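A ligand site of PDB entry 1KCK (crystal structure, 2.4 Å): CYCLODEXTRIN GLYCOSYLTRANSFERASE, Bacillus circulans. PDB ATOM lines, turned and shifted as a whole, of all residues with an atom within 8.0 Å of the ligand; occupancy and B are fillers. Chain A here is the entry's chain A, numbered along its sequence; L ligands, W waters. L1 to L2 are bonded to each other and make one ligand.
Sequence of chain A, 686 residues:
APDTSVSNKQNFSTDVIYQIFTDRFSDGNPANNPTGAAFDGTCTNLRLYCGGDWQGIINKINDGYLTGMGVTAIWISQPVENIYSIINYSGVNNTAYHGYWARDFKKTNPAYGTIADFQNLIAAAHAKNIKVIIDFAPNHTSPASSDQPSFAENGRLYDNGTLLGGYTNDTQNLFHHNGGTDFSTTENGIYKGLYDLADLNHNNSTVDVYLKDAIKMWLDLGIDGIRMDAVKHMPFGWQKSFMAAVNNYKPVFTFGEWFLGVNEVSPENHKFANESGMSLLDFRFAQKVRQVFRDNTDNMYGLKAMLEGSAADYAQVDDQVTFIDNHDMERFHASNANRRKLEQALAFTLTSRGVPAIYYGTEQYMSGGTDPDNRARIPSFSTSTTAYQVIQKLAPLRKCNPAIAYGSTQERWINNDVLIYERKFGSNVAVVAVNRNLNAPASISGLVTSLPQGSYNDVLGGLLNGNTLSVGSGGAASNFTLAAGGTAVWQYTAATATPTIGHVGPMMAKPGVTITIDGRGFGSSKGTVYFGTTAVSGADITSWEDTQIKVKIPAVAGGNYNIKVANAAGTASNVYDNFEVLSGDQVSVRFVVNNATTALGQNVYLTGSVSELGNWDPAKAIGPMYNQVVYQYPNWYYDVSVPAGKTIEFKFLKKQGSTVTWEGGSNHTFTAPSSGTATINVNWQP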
ATOM      1  N   TYR A 301      14.608  30.063 -22.406  1.00  0.00           N
ATOM      2  CA  TYR A 301      15.600  29.836 -23.456  1.00  0.00           C
ATOM      3  C   TYR A 301      16.552  31.024 -23.517  1.00  0.00           C
ATOM      4  O   TYR A 301      17.719  30.881 -23.864  1.00  0.00           O
ATOM      5  CB  TYR A 301      14.906  29.637 -24.809  1.00  0.00           C
ATOM      6  CG  TYR A 301      14.208  28.299 -24.927  1.00  0.00           C
ATOM      7  CD1 TYR A 301      14.943  27.114 -24.978  1.00  0.00           C
ATOM      8  CD2 TYR A 301      12.815  28.204 -24.962  1.00  0.00           C
ATOM      9  CE1 TYR A 301      14.314  25.875 -25.056  1.00  0.00           C
ATOM     10  CE2 TYR A 301      12.174  26.977 -25.037  1.00  0.00           C
ATOM     11  CZ  TYR A 301      12.926  25.814 -25.077  1.00  0.00           C
ATOM     12  OH  TYR A 301      12.301  24.590 -25.136  1.00  0.00           O
ATOM     13  N   LYS A 304      18.898  30.694 -20.562  1.00  0.00           N
ATOM     14  CA  LYS A 304      19.908  29.685 -20.853  1.00  0.00           C
ATOM     15  C   LYS A 304      21.036  30.259 -21.713  1.00  0.00           C
ATOM     16  O   LYS A 304      22.217  30.008 -21.461  1.00  0.00           O
ATOM     17  CB  LYS A 304      19.287  28.494 -21.581  1.00  0.00           C
ATOM     18  CG  LYS A 304      20.322  27.493 -22.100  1.00  0.00           C
ATOM     19  CD  LYS A 304      19.707  26.377 -22.928  1.00  0.00           C
ATOM     20  CE  LYS A 304      20.807  25.512 -23.532  1.00  0.00           C
ATOM     21  NZ  LYS A 304      20.289  24.336 -24.280  1.00  0.00           N
ATOM     22  N   GLN A 410      25.197  23.667 -16.257  1.00  0.00           N
ATOM     23  CA  GLN A 410      24.719  22.905 -17.413  1.00  0.00           C
ATOM     24  C   GLN A 410      23.205  22.718 -17.410  1.00  0.00           C
ATOM     25  O   GLN A 410      22.609  22.339 -16.403  1.00  0.00           O
ATOM     26  CB  GLN A 410      25.390  21.529 -17.462  1.00  0.00           C
ATOM     27  CG  GLN A 410      24.983  20.730 -18.690  1.00  0.00           C
ATOM     28  CD  GLN A 410      25.572  19.336 -18.722  1.00  0.00           C
ATOM     29  OE1 GLN A 410      25.273  18.554 -19.621  1.00  0.00           O
ATOM     30  NE2 GLN A 410      26.404  19.011 -17.742  1.00  0.00           N
ATOM     31  N   GLU A 411      22.592  22.983 -18.564  1.00  0.00           N
ATOM     32  CA  GLU A 411      21.157  22.812 -18.738  1.00  0.00           C
ATOM     33  C   GLU A 411      20.874  21.315 -18.900  1.00  0.00           C
ATOM     34  O   GLU A 411      21.476  20.664 -19.744  1.00  0.00           O
ATOM     35  CB  GLU A 411      20.697  23.598 -19.986  1.00  0.00           C
ATOM     36  CG  GLU A 411      19.249  23.392 -20.400  1.00  0.00           C
ATOM     37  CD  GLU A 411      19.050  22.146 -21.247  1.00  0.00           C
ATOM     38  OE1 GLU A 411      19.677  22.052 -22.327  1.00  0.00           O
ATOM     39  OE2 GLU A 411      18.253  21.275 -20.847  1.00  0.00           O
ATOM     40  N   ARG A 412      19.957  20.791 -18.085  1.00  0.00           N
ATOM     41  CA  ARG A 412      19.627  19.376 -18.157  1.00  0.00           C
ATOM     42  C   ARG A 412      18.174  19.123 -18.558  1.00  0.00           C
ATOM     43  O   ARG A 412      17.806  18.021 -18.946  1.00  0.00           O
ATOM     44  CB  ARG A 412      19.929  18.708 -16.806  1.00  0.00           C
ATOM     45  CG  ARG A 412      21.286  19.119 -16.247  1.00  0.00           C
ATOM     46  CD  ARG A 412      22.162  17.936 -15.863  1.00  0.00           C
ATOM     47  NE  ARG A 412      22.535  17.094 -16.995  1.00  0.00           N
ATOM     48  CZ  ARG A 412      23.529  16.205 -16.971  1.00  0.00           C
ATOM     49  NH1 ARG A 412      24.261  16.058 -15.875  1.00  0.00           N
ATOM     50  NH2 ARG A 412      23.777  15.447 -18.034  1.00  0.00           N
ATOM     51  N   TRP A 413      17.348  20.163 -18.462  1.00  0.00           N
ATOM     52  CA  TRP A 413      15.944  20.075 -18.852  1.00  0.00           C
ATOM     53  C   TRP A 413      15.456  21.509 -19.051  1.00  0.00           C
ATOM     54  O   TRP A 413      15.791  22.400 -18.272  1.00  0.00           O
ATOM     55  CB  TRP A 413      15.117  19.396 -17.773  1.00  0.00           C
ATOM     56  CG  TRP A 413      13.927  18.649 -18.316  1.00  0.00           C
ATOM     57  CD1 TRP A 413      13.869  17.322 -18.646  1.00  0.00           C
ATOM     58  CD2 TRP A 413      12.642  19.193 -18.636  1.00  0.00           C
ATOM     59  NE1 TRP A 413      12.641  17.006 -19.151  1.00  0.00           N
ATOM     60  CE2 TRP A 413      11.853  18.129 -19.157  1.00  0.00           C
ATOM     61  CE3 TRP A 413      12.071  20.468 -18.537  1.00  0.00           C
ATOM     62  CZ2 TRP A 413      10.535  18.316 -19.577  1.00  0.00           C
ATOM     63  CZ3 TRP A 413      10.748  20.648 -18.946  1.00  0.00           C
ATOM     64  CH2 TRP A 413       9.998  19.572 -19.459  1.00  0.00           C
ATOM     65  N   ILE A 414      14.660  21.730 -20.095  1.00  0.00           N
ATOM     66  CA  ILE A 414      14.189  23.081 -20.362  1.00  0.00           C
ATOM     67  C   ILE A 414      13.022  23.182 -21.334  1.00  0.00           C
ATOM     68  O   ILE A 414      12.829  22.325 -22.202  1.00  0.00           O
ATOM     69  CB  ILE A 414      15.363  23.946 -20.904  1.00  0.00           C
ATOM     70  CG1 ILE A 414      14.895  25.377 -21.184  1.00  0.00           C
ATOM     71  CG2 ILE A 414      15.914  23.333 -22.196  1.00  0.00           C
ATOM     72  CD1 ILE A 414      16.004  26.296 -21.668  1.00  0.00           C
ATOM     73  N   ASN A 415      12.229  24.230 -21.161  1.00  0.00           N
ATOM     74  CA  ASN A 415      11.130  24.573 -22.061  1.00  0.00           C
ATOM     75  C   ASN A 415      10.822  26.047 -21.787  1.00  0.00           C
ATOM     76  O   ASN A 415      11.597  26.727 -21.116  1.00  0.00           O
ATOM     77  CB  ASN A 415       9.907  23.661 -21.859  1.00  0.00           C
ATOM     78  CG  ASN A 415       9.129  23.957 -20.589  1.00  0.00           C
ATOM     79  OD1 ASN A 415       9.322  24.982 -19.943  1.00  0.00           O
ATOM     80  ND2 ASN A 415       8.233  23.042 -20.236  1.00  0.00           N
ATOM     81  N   ASN A 416       9.705  26.556 -22.287  1.00  0.00           N
ATOM     82  CA  ASN A 416       9.378  27.965 -22.102  1.00  0.00           C
ATOM     83  C   ASN A 416       9.435  28.474 -20.661  1.00  0.00           C
ATOM     84  O   ASN A 416      10.009  29.523 -20.388  1.00  0.00           O
ATOM     85  CB  ASN A 416       7.998  28.285 -22.667  1.00  0.00           C
ATOM     86  CG  ASN A 416       8.005  28.482 -24.172  1.00  0.00           C
ATOM     87  OD1 ASN A 416       6.987  28.821 -24.758  1.00  0.00           O
ATOM     88  ND2 ASN A 416       9.161  28.254 -24.789  1.00  0.00           N
ATOM     89  N   VAL A 418      10.148  26.245 -17.790  1.00  0.00           N
ATOM     90  CA  VAL A 418      10.933  25.427 -16.875  1.00  0.00           C
ATOM     91  C   VAL A 418      12.423  25.392 -17.197  1.00  0.00           C
ATOM     92  O   VAL A 418      12.824  25.352 -18.360  1.00  0.00           O
ATOM     93  CB  VAL A 418      10.428  23.962 -16.854  1.00  0.00           C
ATOM     94  CG1 VAL A 418      11.225  23.133 -15.862  1.00  0.00           C
ATOM     95  CG2 VAL A 418       8.952  23.936 -16.484  1.00  0.00           C
ATOM     96  N   ILE A 420      15.956  23.447 -15.526  1.00  0.00           N
ATOM     97  CA  ILE A 420      16.616  22.599 -14.538  1.00  0.00           C
ATOM     98  C   ILE A 420      18.095  22.582 -14.915  1.00  0.00           C
ATOM     99  O   ILE A 420      18.458  22.063 -15.974  1.00  0.00           O
ATOM    100  CB  ILE A 420      16.056  21.157 -14.569  1.00  0.00           C
ATOM    101  CG1 ILE A 420      14.556  21.174 -14.278  1.00  0.00           C
ATOM    102  CG2 ILE A 420      16.801  20.298 -13.554  1.00  0.00           C
ATOM    103  CD1 ILE A 420      13.918  19.789 -14.246  1.00  0.00           C
ATOM    104  N   SER A 443       5.239  18.453 -16.390  1.00  0.00           N
ATOM    105  CA  SER A 443       5.546  17.029 -16.333  1.00  0.00           C
ATOM    106  C   SER A 443       6.996  16.811 -16.769  1.00  0.00           C
ATOM    107  O   SER A 443       7.303  16.801 -17.967  1.00  0.00           O
ATOM    108  CB  SER A 443       4.597  16.259 -17.245  1.00  0.00           C
ATOM    109  OG  SER A 443       4.887  14.868 -17.227  1.00  0.00           O
ATOM    110  N   ILE A 444       7.886  16.642 -15.805  1.00  0.00           N
ATOM    111  CA  ILE A 444       9.299  16.437 -16.093  1.00  0.00           C
ATOM    112  C   ILE A 444       9.662  14.964 -16.232  1.00  0.00           C
ATOM    113  O   ILE A 444       9.603  14.203 -15.274  1.00  0.00           O
ATOM    114  CB  ILE A 444      10.214  17.082 -15.008  1.00  0.00           C
ATOM    115  CG1 ILE A 444      10.289  18.598 -15.192  1.00  0.00           C
ATOM    116  CG2 ILE A 444      11.631  16.511 -15.110  1.00  0.00           C
ATOM    117  CD1 ILE A 444       8.998  19.322 -14.977  1.00  0.00           C
ATOM    118  N   SER A 445      10.024  14.567 -17.454  1.00  0.00           N
ATOM    119  CA  SER A 445      10.445  13.199 -17.716  1.00  0.00           C
ATOM    120  C   SER A 445      11.639  13.222 -18.655  1.00  0.00           C
ATOM    121  O   SER A 445      11.714  14.045 -19.571  1.00  0.00           O
ATOM    122  CB  SER A 445       9.283  12.387 -18.330  1.00  0.00           C
ATOM    123  OG  SER A 445       8.739  13.023 -19.474  1.00  0.00           O
ATOM    124  N   GLY A 446      12.601  12.335 -18.410  1.00  0.00           N
ATOM    125  CA  GLY A 446      13.794  12.285 -19.236  1.00  0.00           C
ATOM    126  C   GLY A 446      14.920  13.120 -18.667  1.00  0.00           C
ATOM    127  O   GLY A 446      15.861  13.483 -19.376  1.00  0.00           O
ATOM    128  N   LEU A 447      14.842  13.434 -17.375  1.00  0.00           N
ATOM    129  CA  LEU A 447      15.866  14.222 -16.708  1.00  0.00           C
ATOM    130  C   LEU A 447      17.054  13.339 -16.330  1.00  0.00           C
ATOM    131  O   LEU A 447      16.896  12.320 -15.664  1.00  0.00           O
ATOM    132  CB  LEU A 447      15.304  14.881 -15.446  1.00  0.00           C
ATOM    133  CG  LEU A 447      16.292  15.598 -14.523  1.00  0.00           C
ATOM    134  CD1 LEU A 447      16.939  16.766 -15.257  1.00  0.00           C
ATOM    135  CD2 LEU A 447      15.568  16.080 -13.281  1.00  0.00           C
ATOM    136  N   VAL A 448      18.243  13.752 -16.767  1.00  0.00           N
ATOM    137  CA  VAL A 448      19.470  13.011 -16.464  1.00  0.00           C
ATOM    138  C   VAL A 448      20.382  13.935 -15.649  1.00  0.00           C
ATOM    139  O   VAL A 448      20.506  15.120 -15.954  1.00  0.00           O
ATOM    140  CB  VAL A 448      20.203  12.587 -17.755  1.00  0.00           C
ATOM    141  CG1 VAL A 448      21.482  11.839 -17.418  1.00  0.00           C
ATOM    142  CG2 VAL A 448      19.295  11.705 -18.605  1.00  0.00           C
HETATM  143  C1  LIG L   1      11.635  17.674 -22.985  1.00  0.00           C
HETATM  144  C2  LIG L   1      12.444  18.888 -22.516  1.00  0.00           C
HETATM  145  C3  LIG L   1      13.919  18.719 -22.880  1.00  0.00           C
HETATM  146  C4  LIG L   1      14.451  17.380 -22.357  1.00  0.00           C
HETATM  147  C5  LIG L   1      13.560  16.247 -22.863  1.00  0.00           C
HETATM  148  C6  LIG L   1      13.984  14.896 -22.311  1.00  0.00           C
HETATM  149  O1  LIG L   1      11.660  17.602 -24.365  1.00  0.00           O
HETATM  150  O2  LIG L   1      11.944  20.066 -23.120  1.00  0.00           O
HETATM  151  O3  LIG L   1      14.683  19.775 -22.322  1.00  0.00           O
HETATM  152  O4  LIG L   1      15.803  17.186 -22.817  1.00  0.00           O
HETATM  153  O5  LIG L   1      12.184  16.462 -22.451  1.00  0.00           O
HETATM  154  O6  LIG L   1      13.103  13.869 -22.734  1.00  0.00           O
HETATM  155  C1  LG2 L   2      16.770  17.096 -21.804  1.00  0.00           C
HETATM  156  C2  LG2 L   2      17.984  17.963 -22.174  1.00  0.00           C
HETATM  157  C3  LG2 L   2      18.689  17.375 -23.391  1.00  0.00           C
HETATM  158  C4  LG2 L   2      19.059  15.906 -23.137  1.00  0.00           C
HETATM  159  C5  LG2 L   2      17.828  15.112 -22.696  1.00  0.00           C
HETATM  160  C6  LG2 L   2      18.150  13.697 -22.265  1.00  0.00           C
HETATM  161  O1  LG2 L   2      17.563  19.293 -22.460  1.00  0.00           O
HETATM  162  O2  LG2 L   2      19.859  18.125 -23.674  1.00  0.00           O
HETATM  163  O3  LG2 L   2      19.593  15.343 -24.328  1.00  0.00           O
HETATM  164  O4  LG2 L   2      17.187  15.754 -21.561  1.00  0.00           O
HETATM  165  O5  LG2 L   2      16.974  12.957 -22.021  1.00  0.00           O
HETATM  166  O   HOH W   1      21.401  18.312 -21.222  1.00  0.00           O
HETATM  167  O   HOH W   2      22.296  15.649 -24.024  1.00  0.00           O
HETATM  168  O   HOH W   3      16.604  20.081 -25.316  1.00  0.00           O
HETATM  169  O   HOH W   4      13.405  22.217 -25.045  1.00  0.00           O
HETATM  170  O   HOH W   5      18.583  15.446 -19.032  1.00  0.00           O
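Water W1 lies within hydrogen-bond range of the backbone carbonyl oxygen of Glu 411 (2.8 Å) and an oxygen (O2) of LG2 L2 (2.9 Å).
Water W4 lies within hydrogen-bond range of the side-chain hydroxyl of Tyr 301 (2.6 Å), the backbone carbonyl oxygen of Ile 414 (2.9 Å) and an oxygen (O2) of LIG L1 (3.2 Å).
Merely in contact with the ligand: Arg 412 (3.2 Å).
Six residues have an atom within 4 Å of the ligand: Glu 411, Arg 412, Trp 413, Ile 414, Ser 445 and Gly 446.
The side-chain carboxylate (OE2) of Glu 411 is in hydrogen-bond range of the backbone NH (N) of Trp 413, at 2.8 Å.
O of Trp 413 is in hydrogen-bond range of N of Ile 420 (2.9 Å).
NE1 of Trp 413 lies within hydrogen-bond range of O of Ser 445 (3.1 Å).
The backbone NH of Arg 412 lies within hydrogen-bond range of the backbone carbonyl oxygen of Ile 420 (2.9 Å).
O of Val 448 is in hydrogen-bond range of NE of Arg 412, at 3.0 Å.
The side-chain amino group (NZ) of Lys 304 is in salt-bridge range of the side-chain carboxylate (OE1) of Glu 411, at 3.1 Å.
The backbone carbonyl oxygen of Ser 445 is in hydrogen-bond range of an oxygen (O6) of LIG L1, 3.5 Å away.
The indole nitrogen of Trp 413 sits at hydrogen-bond distance from an oxygen (O5) of LIG L1, 3.4 Å away.
O2 of LIG L1 is in hydrogen-bond range of O of Ile 414 (2.6 Å).
OE2 of Glu 411 sits at hydrogen-bond distance from O1 of LG2 L2.
O5 of LG2 L2 sits at hydrogen-bond distance from O of Gly 446.
The backbone NH (N) of Ile 414 is in hydrogen-bond range of an oxygen (O3) of LIG L1 (3.0 Å).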
